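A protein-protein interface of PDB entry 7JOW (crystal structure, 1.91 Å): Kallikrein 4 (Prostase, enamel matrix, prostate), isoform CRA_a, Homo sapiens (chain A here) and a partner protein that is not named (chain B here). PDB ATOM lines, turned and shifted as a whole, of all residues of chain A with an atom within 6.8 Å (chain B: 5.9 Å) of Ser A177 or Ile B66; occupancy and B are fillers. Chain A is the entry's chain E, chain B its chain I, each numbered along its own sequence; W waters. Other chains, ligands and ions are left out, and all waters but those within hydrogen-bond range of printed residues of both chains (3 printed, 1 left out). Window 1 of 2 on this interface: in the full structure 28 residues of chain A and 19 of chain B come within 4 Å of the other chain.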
ATOM      1  N   LEU A  18      13.530  -3.107   3.109  1.00  0.00           N
ATOM      2  CA  LEU A  18      12.577  -2.596   2.093  1.00  0.00           C
ATOM      3  C   LEU A  18      13.373  -2.342   0.815  1.00  0.00           C
ATOM      4  O   LEU A  18      14.365  -1.569   0.817  1.00  0.00           O
ATOM      5  CB  LEU A  18      11.819  -1.357   2.589  1.00  0.00           C
ATOM      6  CG  LEU A  18      10.598  -1.578   3.475  1.00  0.00           C
ATOM      7  CD1 LEU A  18      10.870  -2.362   4.707  1.00  0.00           C
ATOM      8  CD2 LEU A  18      10.091  -0.215   3.902  1.00  0.00           C
ATOM      9  N   PHE A  25      16.186   0.551   0.211  1.00  0.00           N
ATOM     10  CA  PHE A  25      16.136   2.040   0.469  1.00  0.00           C
ATOM     11  C   PHE A  25      15.808   2.379   1.929  1.00  0.00           C
ATOM     12  O   PHE A  25      16.159   3.548   2.313  1.00  0.00           O
ATOM     13  CB  PHE A  25      15.114   2.715  -0.450  1.00  0.00           C
ATOM     14  CG  PHE A  25      13.706   2.202  -0.286  1.00  0.00           C
ATOM     15  CD1 PHE A  25      13.304   1.029  -0.920  1.00  0.00           C
ATOM     16  CD2 PHE A  25      12.777   2.911   0.456  1.00  0.00           C
ATOM     17  CE1 PHE A  25      11.996   0.604  -0.790  1.00  0.00           C
ATOM     18  CE2 PHE A  25      11.482   2.457   0.638  1.00  0.00           C
ATOM     19  CZ  PHE A  25      11.100   1.300   0.013  1.00  0.00           C
ATOM     20  N   CYS A  26      15.254   1.439   2.689  1.00  0.00           N
ATOM     21  CA  CYS A  26      14.831   1.589   4.124  1.00  0.00           C
ATOM     22  C   CYS A  26      14.890   0.210   4.768  1.00  0.00           C
ATOM     23  O   CYS A  26      14.892  -0.796   4.039  1.00  0.00           O
ATOM     24  CB  CYS A  26      13.360   2.098   4.238  1.00  0.00           C
ATOM     25  SG  CYS A  26      13.258   3.908   4.057  1.00  0.00           S
ATOM     26  N   SER A  27      14.820   0.146   6.083  1.00  0.00           N
ATOM     27  CA  SER A  27      14.546  -1.074   6.853  1.00  0.00           C
ATOM     28  C   SER A  27      13.164  -0.880   7.495  1.00  0.00           C
ATOM     29  O   SER A  27      12.523   0.177   7.349  1.00  0.00           O
ATOM     30  CB  SER A  27      15.702  -1.432   7.871  1.00  0.00           C
ATOM     31  OG  SER A  27      16.913  -1.825   7.109  1.00  0.00           O
ATOM     32  N   GLY A  28      12.769  -1.908   8.193  1.00  0.00           N
ATOM     33  CA  GLY A  28      11.623  -2.039   9.074  1.00  0.00           C
ATOM     34  C   GLY A  28      11.926  -3.101  10.093  1.00  0.00           C
ATOM     35  O   GLY A  28      13.080  -3.640  10.122  1.00  0.00           O
ATOM     36  N   SER A  38       7.896   0.561  10.181  1.00  0.00           N
ATOM     37  CA  SER A  38       8.942   1.341   9.500  1.00  0.00           C
ATOM     38  C   SER A  38       8.640   2.808   9.720  1.00  0.00           C
ATOM     39  O   SER A  38       7.688   3.140  10.400  1.00  0.00           O
ATOM     40  CB  SER A  38       9.042   0.968   8.006  1.00  0.00           C
ATOM     41  OG  SER A  38      10.263   1.481   7.465  1.00  0.00           O
ATOM     42  N   ALA A  39       9.536   3.649   9.239  1.00  0.00           N
ATOM     43  CA  ALA A  39       9.386   5.115   9.238  1.00  0.00           C
ATOM     44  C   ALA A  39       8.311   5.465   8.191  1.00  0.00           C
ATOM     45  O   ALA A  39       8.250   4.868   7.103  1.00  0.00           O
ATOM     46  CB  ALA A  39      10.679   5.748   8.900  1.00  0.00           C
ATOM     47  N   HIS A  41       8.258   8.092   6.474  1.00  0.00           N
ATOM     48  CA  HIS A  41       8.782   8.776   5.263  1.00  0.00           C
ATOM     49  C   HIS A  41       9.197   7.749   4.204  1.00  0.00           C
ATOM     50  O   HIS A  41       9.598   8.156   3.075  1.00  0.00           O
ATOM     51  CB  HIS A  41       9.950   9.686   5.717  1.00  0.00           C
ATOM     52  CG  HIS A  41      11.220   9.026   6.158  1.00  0.00           C
ATOM     53  ND1 HIS A  41      11.543   8.882   7.510  1.00  0.00           N
ATOM     54  CD2 HIS A  41      12.270   8.567   5.488  1.00  0.00           C
ATOM     55  CE1 HIS A  41      12.747   8.393   7.631  1.00  0.00           C
ATOM     56  NE2 HIS A  41      13.239   8.132   6.375  1.00  0.00           N
ATOM     57  N   CYS A  42       9.320   6.488   4.610  1.00  0.00           N
ATOM     58  CA  CYS A  42       9.633   5.361   3.655  1.00  0.00           C
ATOM     59  C   CYS A  42       8.420   4.832   2.878  1.00  0.00           C
ATOM     60  O   CYS A  42       8.569   3.828   2.188  1.00  0.00           O
ATOM     61  CB  CYS A  42      10.236   4.156   4.396  1.00  0.00           C
ATOM     62  SG  CYS A  42      11.774   4.572   5.268  1.00  0.00           S
ATOM     63  N   PHE A  43       7.246   5.386   3.106  1.00  0.00           N
ATOM     64  CA  PHE A  43       5.964   5.008   2.455  1.00  0.00           C
ATOM     65  C   PHE A  43       6.169   4.781   0.955  1.00  0.00           C
ATOM     66  O   PHE A  43       6.721   5.660   0.236  1.00  0.00           O
ATOM     67  CB  PHE A  43       4.923   6.101   2.636  1.00  0.00           C
ATOM     68  CG  PHE A  43       3.635   5.752   1.920  1.00  0.00           C
ATOM     69  CD1 PHE A  43       2.701   4.897   2.496  1.00  0.00           C
ATOM     70  CD2 PHE A  43       3.449   6.159   0.625  1.00  0.00           C
ATOM     71  CE1 PHE A  43       1.547   4.529   1.791  1.00  0.00           C
ATOM     72  CE2 PHE A  43       2.290   5.795  -0.088  1.00  0.00           C
ATOM     73  CZ  PHE A  43       1.302   5.031   0.518  1.00  0.00           C
ATOM     74  N   ASP A  86       6.881   9.801  13.170  1.00  0.00           N
ATOM     75  CA  ASP A  86       7.399   9.206  11.924  1.00  0.00           C
ATOM     76  C   ASP A  86       7.357   7.680  12.009  1.00  0.00           C
ATOM     77  O   ASP A  86       8.462   7.035  12.356  1.00  0.00           O
ATOM     78  CB  ASP A  86       8.845   9.666  11.717  1.00  0.00           C
ATOM     79  CG  ASP A  86       9.432   9.251  10.366  1.00  0.00           C
ATOM     80  OD1 ASP A  86       8.667   8.687   9.503  1.00  0.00           O
ATOM     81  OD2 ASP A  86      10.668   9.531  10.106  1.00  0.00           O
ATOM     82  N   GLY A 124      22.627   0.715   5.750  1.00  0.00           N
ATOM     83  CA  GLY A 124      22.905   2.042   5.175  1.00  0.00           C
ATOM     84  C   GLY A 124      24.377   2.328   4.982  1.00  0.00           C
ATOM     85  O   GLY A 124      25.221   1.512   5.304  1.00  0.00           O
ATOM     86  N   SER A 172      23.508   6.395  12.773  1.00  0.00           N
ATOM     87  CA  SER A 172      22.778   5.925  11.568  1.00  0.00           C
ATOM     88  C   SER A 172      23.166   6.772  10.368  1.00  0.00           C
ATOM     89  O   SER A 172      23.515   7.969  10.518  1.00  0.00           O
ATOM     90  CB  SER A 172      21.312   6.107  11.768  1.00  0.00           C
ATOM     91  OG  SER A 172      20.902   5.318  12.853  1.00  0.00           O
ATOM     92  N   CYS A 173      22.962   6.241   9.185  1.00  0.00           N
ATOM     93  CA  CYS A 173      23.244   6.993   7.942  1.00  0.00           C
ATOM     94  C   CYS A 173      22.197   6.591   6.871  1.00  0.00           C
ATOM     95  O   CYS A 173      21.229   5.927   7.175  1.00  0.00           O
ATOM     96  CB  CYS A 173      24.723   6.888   7.503  1.00  0.00           C
ATOM     97  SG  CYS A 173      25.120   8.192   6.256  1.00  0.00           S
ATOM     98  N   ASN A 174      22.355   7.074   5.652  1.00  0.00           N
ATOM     99  CA  ASN A 174      21.273   7.001   4.627  1.00  0.00           C
ATOM    100  C   ASN A 174      21.069   5.538   4.261  1.00  0.00           C
ATOM    101  O   ASN A 174      22.056   4.903   3.861  1.00  0.00           O
ATOM    102  CB  ASN A 174      21.616   7.880   3.429  1.00  0.00           C
ATOM    103  CG  ASN A 174      21.544   9.371   3.740  1.00  0.00           C
ATOM    104  OD1 ASN A 174      20.887   9.798   4.714  1.00  0.00           O
ATOM    105  ND2 ASN A 174      22.002  10.183   2.811  1.00  0.00           N
ATOM    106  N   GLY A 175      19.832   5.068   4.310  1.00  0.00           N
ATOM    107  CA  GLY A 175      19.476   3.665   4.092  1.00  0.00           C
ATOM    108  C   GLY A 175      19.166   2.956   5.393  1.00  0.00           C
ATOM    109  O   GLY A 175      18.584   1.884   5.305  1.00  0.00           O
ATOM    110  N   ASP A 176      19.435   3.597   6.557  1.00  0.00           N
ATOM    111  CA  ASP A 176      19.145   2.983   7.873  1.00  0.00           C
ATOM    112  C   ASP A 176      17.750   3.365   8.381  1.00  0.00           C
ATOM    113  O   ASP A 176      17.230   2.694   9.307  1.00  0.00           O
ATOM    114  CB  ASP A 176      20.188   3.428   8.892  1.00  0.00           C
ATOM    115  CG  ASP A 176      21.546   2.825   8.606  1.00  0.00           C
ATOM    116  OD1 ASP A 176      21.624   1.610   8.227  1.00  0.00           O
ATOM    117  OD2 ASP A 176      22.553   3.556   8.909  1.00  0.00           O
ATOM    118  N   SER A 177      17.097   4.335   7.728  1.00  0.00           N
ATOM    119  CA  SER A 177      15.723   4.740   8.068  1.00  0.00           C
ATOM    120  C   SER A 177      14.865   3.523   8.290  1.00  0.00           C
ATOM    121  O   SER A 177      14.839   2.628   7.423  1.00  0.00           O
ATOM    122  CB  SER A 177      15.073   5.651   7.004  1.00  0.00           C
ATOM    123  OG  SER A 177      15.440   6.987   7.216  1.00  0.00           O
ATOM    124  N   GLY A 178      14.073   3.581   9.356  1.00  0.00           N
ATOM    125  CA  GLY A 178      13.017   2.600   9.642  1.00  0.00           C
ATOM    126  C   GLY A 178      13.521   1.378  10.388  1.00  0.00           C
ATOM    127  O   GLY A 178      12.667   0.586  10.876  1.00  0.00           O
ATOM    128  N   GLY A 179      14.816   1.207  10.475  1.00  0.00           N
ATOM    129  CA  GLY A 179      15.378   0.119  11.246  1.00  0.00           C
ATOM    130  C   GLY A 179      15.408   0.357  12.751  1.00  0.00           C
ATOM    131  O   GLY A 179      15.098   1.442  13.275  1.00  0.00           O
ATOM    132  N   PRO A 180      15.704  -0.745  13.457  1.00  0.00           N
ATOM    133  CA  PRO A 180      15.489  -0.832  14.897  1.00  0.00           C
ATOM    134  C   PRO A 180      16.566  -0.150  15.762  1.00  0.00           C
ATOM    135  O   PRO A 180      17.754  -0.223  15.473  1.00  0.00           O
ATOM    136  CB  PRO A 180      15.461  -2.353  15.145  1.00  0.00           C
ATOM    137  CG  PRO A 180      16.471  -2.873  14.145  1.00  0.00           C
ATOM    138  CD  PRO A 180      16.174  -2.026  12.879  1.00  0.00           C
ATOM    139  N   LEU A 190      12.799   3.782  16.066  1.00  0.00           N
ATOM    140  CA  LEU A 190      13.098   3.586  14.615  1.00  0.00           C
ATOM    141  C   LEU A 190      14.044   4.694  14.177  1.00  0.00           C
ATOM    142  O   LEU A 190      13.870   5.878  14.560  1.00  0.00           O
ATOM    143  CB  LEU A 190      11.841   3.616  13.767  1.00  0.00           C
ATOM    144  CG  LEU A 190      10.709   2.723  14.203  1.00  0.00           C
ATOM    145  CD1 LEU A 190       9.457   3.044  13.360  1.00  0.00           C
ATOM    146  CD2 LEU A 190      11.036   1.280  14.000  1.00  0.00           C
ATOM    147  N   VAL A 191      15.011   4.350  13.368  1.00  0.00           N
ATOM    148  CA  VAL A 191      15.841   5.392  12.730  1.00  0.00           C
ATOM    149  C   VAL A 191      14.930   6.378  11.959  1.00  0.00           C
ATOM    150  O   VAL A 191      14.107   5.904  11.100  1.00  0.00           O
ATOM    151  CB  VAL A 191      16.868   4.730  11.792  1.00  0.00           C
ATOM    152  CG1 VAL A 191      17.746   5.754  11.108  1.00  0.00           C
ATOM    153  CG2 VAL A 191      17.757   3.760  12.557  1.00  0.00           C
ATOM    154  N   SER A 192      15.125   7.684  12.186  1.00  0.00           N
ATOM    155  CA  SER A 192      14.258   8.730  11.568  1.00  0.00           C
ATOM    156  C   SER A 192      15.126   9.715  10.790  1.00  0.00           C
ATOM    157  O   SER A 192      15.113   9.699   9.502  1.00  0.00           O
ATOM    158  CB  SER A 192      13.352   9.362  12.583  1.00  0.00           C
ATOM    159  OG  SER A 192      12.378  10.249  11.972  1.00  0.00           O
ATOM    160  N   PHE A 193      15.877  10.585  11.442  1.00  0.00           N
ATOM    161  CA  PHE A 193      16.550  11.696  10.731  1.00  0.00           C
ATOM    162  C   PHE A 193      17.700  12.207  11.567  1.00  0.00           C
ATOM    163  O   PHE A 193      17.831  11.813  12.655  1.00  0.00           O
ATOM    164  CB  PHE A 193      15.595  12.852  10.352  1.00  0.00           C
ATOM    165  CG  PHE A 193      15.145  13.718  11.492  1.00  0.00           C
ATOM    166  CD1 PHE A 193      14.062  13.356  12.240  1.00  0.00           C
ATOM    167  CD2 PHE A 193      15.880  14.812  11.868  1.00  0.00           C
ATOM    168  CE1 PHE A 193      13.633  14.139  13.311  1.00  0.00           C
ATOM    169  CE2 PHE A 193      15.483  15.566  12.939  1.00  0.00           C
ATOM    170  CZ  PHE A 193      14.356  15.230  13.653  1.00  0.00           C
ATOM    171  N   ASN B  15      19.990  10.520  -1.976  1.00  0.00           N
ATOM    172  CA  ASN B  15      19.970  11.548  -0.912  1.00  0.00           C
ATOM    173  C   ASN B  15      21.411  11.948  -0.607  1.00  0.00           C
ATOM    174  O   ASN B  15      22.040  11.310   0.243  1.00  0.00           O
ATOM    175  CB  ASN B  15      19.185  11.086   0.307  1.00  0.00           C
ATOM    176  CG  ASN B  15      19.089  12.074   1.454  1.00  0.00           C
ATOM    177  OD1 ASN B  15      19.531  13.234   1.315  1.00  0.00           O
ATOM    178  ND2 ASN B  15      18.471  11.590   2.537  1.00  0.00           N
ATOM    179  N   SER B  62      18.146  15.622   2.094  1.00  0.00           N
ATOM    180  CA  SER B  62      17.136  15.533   3.150  1.00  0.00           C
ATOM    181  C   SER B  62      17.807  15.084   4.458  1.00  0.00           C
ATOM    182  O   SER B  62      18.637  14.193   4.415  1.00  0.00           O
ATOM    183  CB  SER B  62      16.057  14.570   2.778  1.00  0.00           C
ATOM    184  OG  SER B  62      15.196  14.330   3.858  1.00  0.00           O
ATOM    185  N   LEU B  64      16.309  13.144   6.511  1.00  0.00           N
ATOM    186  CA  LEU B  64      15.804  11.772   6.610  1.00  0.00           C
ATOM    187  C   LEU B  64      16.930  10.760   6.262  1.00  0.00           C
ATOM    188  O   LEU B  64      17.645  10.989   5.347  1.00  0.00           O
ATOM    189  CB  LEU B  64      14.596  11.584   5.685  1.00  0.00           C
ATOM    190  CG  LEU B  64      13.397  12.544   5.943  1.00  0.00           C
ATOM    191  CD1 LEU B  64      12.405  12.393   4.789  1.00  0.00           C
ATOM    192  CD2 LEU B  64      12.801  12.281   7.340  1.00  0.00           C
ATOM    193  N   ARG B  65      17.036   9.676   6.994  1.00  0.00           N
ATOM    194  CA  ARG B  65      18.108   8.648   6.789  1.00  0.00           C
ATOM    195  C   ARG B  65      17.740   7.625   5.684  1.00  0.00           C
ATOM    196  O   ARG B  65      18.189   6.427   5.720  1.00  0.00           O
ATOM    197  CB  ARG B  65      18.370   7.953   8.109  1.00  0.00           C
ATOM    198  CG  ARG B  65      19.007   8.837   9.150  1.00  0.00           C
ATOM    199  CD  ARG B  65      20.012   9.844   8.648  1.00  0.00           C
ATOM    200  NE  ARG B  65      20.773  10.461   9.760  1.00  0.00           N
ATOM    201  CZ  ARG B  65      21.420  11.621   9.614  1.00  0.00           C
ATOM    202  NH1 ARG B  65      21.280  12.371   8.498  1.00  0.00           N
ATOM    203  NH2 ARG B  65      22.135  12.060  10.644  1.00  0.00           N
ATOM    204  N   ILE B  66      17.064   8.089   4.651  1.00  0.00           N
ATOM    205  CA  ILE B  66      16.645   7.266   3.470  1.00  0.00           C
ATOM    206  C   ILE B  66      17.645   7.604   2.381  1.00  0.00           C
ATOM    207  O   ILE B  66      18.191   8.730   2.437  1.00  0.00           O
ATOM    208  CB  ILE B  66      15.169   7.549   3.113  1.00  0.00           C
ATOM    209  CG1 ILE B  66      14.646   6.615   2.028  1.00  0.00           C
ATOM    210  CG2 ILE B  66      14.991   8.986   2.716  1.00  0.00           C
ATOM    211  CD1 ILE B  66      13.206   6.737   1.814  1.00  0.00           C
ATOM    212  N   ASN B  67      17.951   6.681   1.462  1.00  0.00           N
ATOM    213  CA  ASN B  67      18.981   6.892   0.419  1.00  0.00           C
ATOM    214  C   ASN B  67      18.387   7.366  -0.941  1.00  0.00           C
ATOM    215  O   ASN B  67      19.168   7.452  -1.924  1.00  0.00           O
ATOM    216  CB  ASN B  67      19.934   5.651   0.307  1.00  0.00           C
ATOM    217  CG  ASN B  67      19.228   4.366  -0.112  1.00  0.00           C
ATOM    218  OD1 ASN B  67      19.838   3.205  -0.115  1.00  0.00           O
ATOM    219  ND2 ASN B  67      17.982   4.491  -0.541  1.00  0.00           N
ATOM    220  N   ILE B  68      17.098   7.743  -0.991  1.00  0.00           N
ATOM    221  CA  ILE B  68      16.451   8.285  -2.209  1.00  0.00           C
ATOM    222  C   ILE B  68      15.669   9.523  -1.844  1.00  0.00           C
ATOM    223  O   ILE B  68      15.445   9.743  -0.665  1.00  0.00           O
ATOM    224  CB  ILE B  68      15.541   7.199  -2.804  1.00  0.00           C
ATOM    225  CG1 ILE B  68      14.437   6.899  -1.823  1.00  0.00           C
ATOM    226  CG2 ILE B  68      16.316   5.950  -3.172  1.00  0.00           C
ATOM    227  CD1 ILE B  68      13.494   5.867  -2.243  1.00  0.00           C
ATOM    228  N   ILE B  69      15.230  10.256  -2.842  1.00  0.00           N
ATOM    229  CA  ILE B  69      14.490  11.531  -2.765  1.00  0.00           C
ATOM    230  C   ILE B  69      13.109  11.262  -3.309  1.00  0.00           C
ATOM    231  O   ILE B  69      12.933  10.836  -4.517  1.00  0.00           O
ATOM    232  CB  ILE B  69      15.281  12.568  -3.575  1.00  0.00           C
ATOM    233  CG1 ILE B  69      16.652  12.819  -2.958  1.00  0.00           C
ATOM    234  CG2 ILE B  69      14.533  13.839  -3.706  1.00  0.00           C
ATOM    235  CD1 ILE B  69      16.601  13.251  -1.559  1.00  0.00           C
ATOM    236  N   LYS B  70      12.147  11.670  -2.535  1.00  0.00           N
ATOM    237  CA  LYS B  70      10.752  11.702  -3.004  1.00  0.00           C
ATOM    238  C   LYS B  70      10.308  13.132  -3.323  1.00  0.00           C
ATOM    239  O   LYS B  70      10.914  14.110  -2.809  1.00  0.00           O
ATOM    240  CB  LYS B  70       9.817  11.119  -1.979  1.00  0.00           C
ATOM    241  CG  LYS B  70      10.069   9.664  -1.671  1.00  0.00           C
ATOM    242  CD  LYS B  70       8.739   9.171  -1.163  1.00  0.00           C
ATOM    243  CE  LYS B  70       8.691   8.275   0.035  1.00  0.00           C
ATOM    244  NZ  LYS B  70       7.486   8.611   0.785  1.00  0.00           N
ATOM    245  N   TYR B  73       9.465  15.548  -0.389  1.00  0.00           N
ATOM    246  CA  TYR B  73      10.446  15.979   0.602  1.00  0.00           C
ATOM    247  C   TYR B  73      10.846  17.440   0.418  1.00  0.00           C
ATOM    248  O   TYR B  73      11.227  17.825  -0.662  1.00  0.00           O
ATOM    249  CB  TYR B  73      11.712  15.149   0.538  1.00  0.00           C
ATOM    250  CG  TYR B  73      11.633  13.693   0.925  1.00  0.00           C
ATOM    251  CD1 TYR B  73      10.524  13.160   1.545  1.00  0.00           C
ATOM    252  CD2 TYR B  73      12.713  12.829   0.627  1.00  0.00           C
ATOM    253  CE1 TYR B  73      10.458  11.814   1.826  1.00  0.00           C
ATOM    254  CE2 TYR B  73      12.663  11.497   0.941  1.00  0.00           C
ATOM    255  CZ  TYR B  73      11.552  11.010   1.564  1.00  0.00           C
ATOM    256  OH  TYR B  73      11.527   9.715   1.926  1.00  0.00           O
HETATM  257  O   HOH W   1      21.044   9.681  12.246  1.00  0.00           O
HETATM  258  O   HOH W   2      21.895   8.555   0.029  1.00  0.00           O
HETATM  259  O   HOH W   3      21.636  13.354   3.285  1.00  0.00           O
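Water W1 lies within hydrogen-bond range of the guanidinium group (NE) of Arg B65 (2.6 Å) and the backbone carbonyl oxygen (O) of Ser A172 (3.5 Å). Water W2 lies within hydrogen-bond range of O of Asn B15 and ND2 of Asn A174. Water W3 lies within hydrogen-bond range of OD1 of Asn B15 (2.9 Å), ND2 of Asn A174 (3.2 Å) and O of Ser B62 (3.3 Å).
Of the 25 printed residues of chain A, 13 touch a printed residue of chain B. Printed residues of chain A that touch a printed residue of chain B: Phe A25, Cys A26, His A41, Phe A43, Ser A172, Cys A173, Asn A174, Gly A175, Asp A176, Ser A177, Val A191, Ser A192 and Phe A193. Hydrophobic or aromatic side chains of chain A that line the printed part of chain B: Phe A25, His A41, Val A191 and Phe A193. Hydrophobic or aromatic side chains of chain B that line the printed part of chain A: Leu B64, Ile B66, Ile B68 and Tyr B73. Along chain B the printed residues that touch a printed residue of chain A span positions 15 to 73. Among the printed residues, 26 pairs touch across the chains.
Of chain B, only Arg B65 (2.8 Å) and Ile B66 (3.2 Å) come within 4 Å of Ser A177. Printed residues of chain A within 4 Å of Ile B68: Phe A25. Of the printed residues of chain A, Arg B65 touches Ser A172, Cys A173, Asn A174, Gly A175, Asp A176, Ser A177, Val A191, Ser A192 and Phe A193. Asp A86 touches none of the printed residues of chain B. Ser B62 touches none of the printed residues of chain A. The nearest residue of chain A that does not touch Ile B66 is Cys A42 (4.2 Å). The nearest printed residue of chain B that does not touch Ser A192 is Ile B66 (5.5 Å).
N of Gly A178 sits at hydrogen-bond distance from O of Val A191 (2.9 Å). The side-chain amide nitrogen (ND2) of Asn B15 is in hydrogen-bond range of the backbone carbonyl oxygen (O) of Leu B64, 3.0 Å away. A ring nitrogen (ND1) of His A41 sits at hydrogen-bond distance from the side-chain carboxylate (OD2) of Asp A86, 2.8 Å away. N of Gly A124 is in hydrogen-bond range of OD1 of Asp A176 (2.8 Å). OD1 of Asn B15 is in hydrogen-bond range of N of Ser B62. N of Leu A18 sits at hydrogen-bond distance from O of Cys A26 (2.8 Å).
Among the printed residues, pairs that only touch across the chains: Phe A25 with Ile B66 (3.4 Å), Phe A25 with Asn B67 (3.2 Å), Phe A25 with Ile B68 (3.97 Å), Cys A26 with Ile B66 (3.6 Å), His A41 with Leu B64 (3.6 Å), His A41 with Ile B66 (3.8 Å), Ser A172 with Arg B65 (3.8 Å), Asn A174 with Leu B64 (3.5 Å), Asn A174 with Arg B65 (3.3 Å), Asn A174 with Ile B66 (3.7 Å), Gly A175 with Ile B66 (3.9 Å), Gly A175 with Asn B67 (3.8 Å), Val A191 with Arg B65 (3.8 Å), Ser A192 with Leu B64 (3.6 Å), Phe A193 with Leu B64 (3.9 Å) and Phe A193 with Arg B65 (3.97 Å).
The side-chain hydroxyl of Ser A177 is in hydrogen-bond range of the backbone NH of Ile B66 (3.2 Å). The backbone carbonyl oxygen (O) of Arg B65 lies within hydrogen-bond range of the backbone NH (N) of Asp A176, at 3.2 Å. The backbone carbonyl oxygen of His A41 lies within hydrogen-bond range of the side-chain hydroxyl of Tyr B73 (2.7 Å). The side-chain amino group (NZ) of Lys B70 is in hydrogen-bond range of the backbone carbonyl oxygen (O) of Phe A43 (3.1 Å). O of Ser A192 sits at hydrogen-bond distance from N of Arg B65 (3.2 Å). N of Gly A175 sits at hydrogen-bond distance from O of Arg B65. The side-chain amide nitrogen of Asn A174 sits at hydrogen-bond distance from the backbone carbonyl oxygen of Asn B15. The backbone carbonyl oxygen (O) of Cys A173 sits close to the backbone carbonyl oxygen (O) of Arg B65, at 3.4 Å. The backbone carbonyl oxygen (O) of Arg B65 sits at hydrogen-bond distance from the backbone NH (N) of Ser A177. The side-chain amino group (NZ) of Lys B70 lies within hydrogen-bond range of the backbone carbonyl oxygen (O) of His A41 (3.1 Å).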
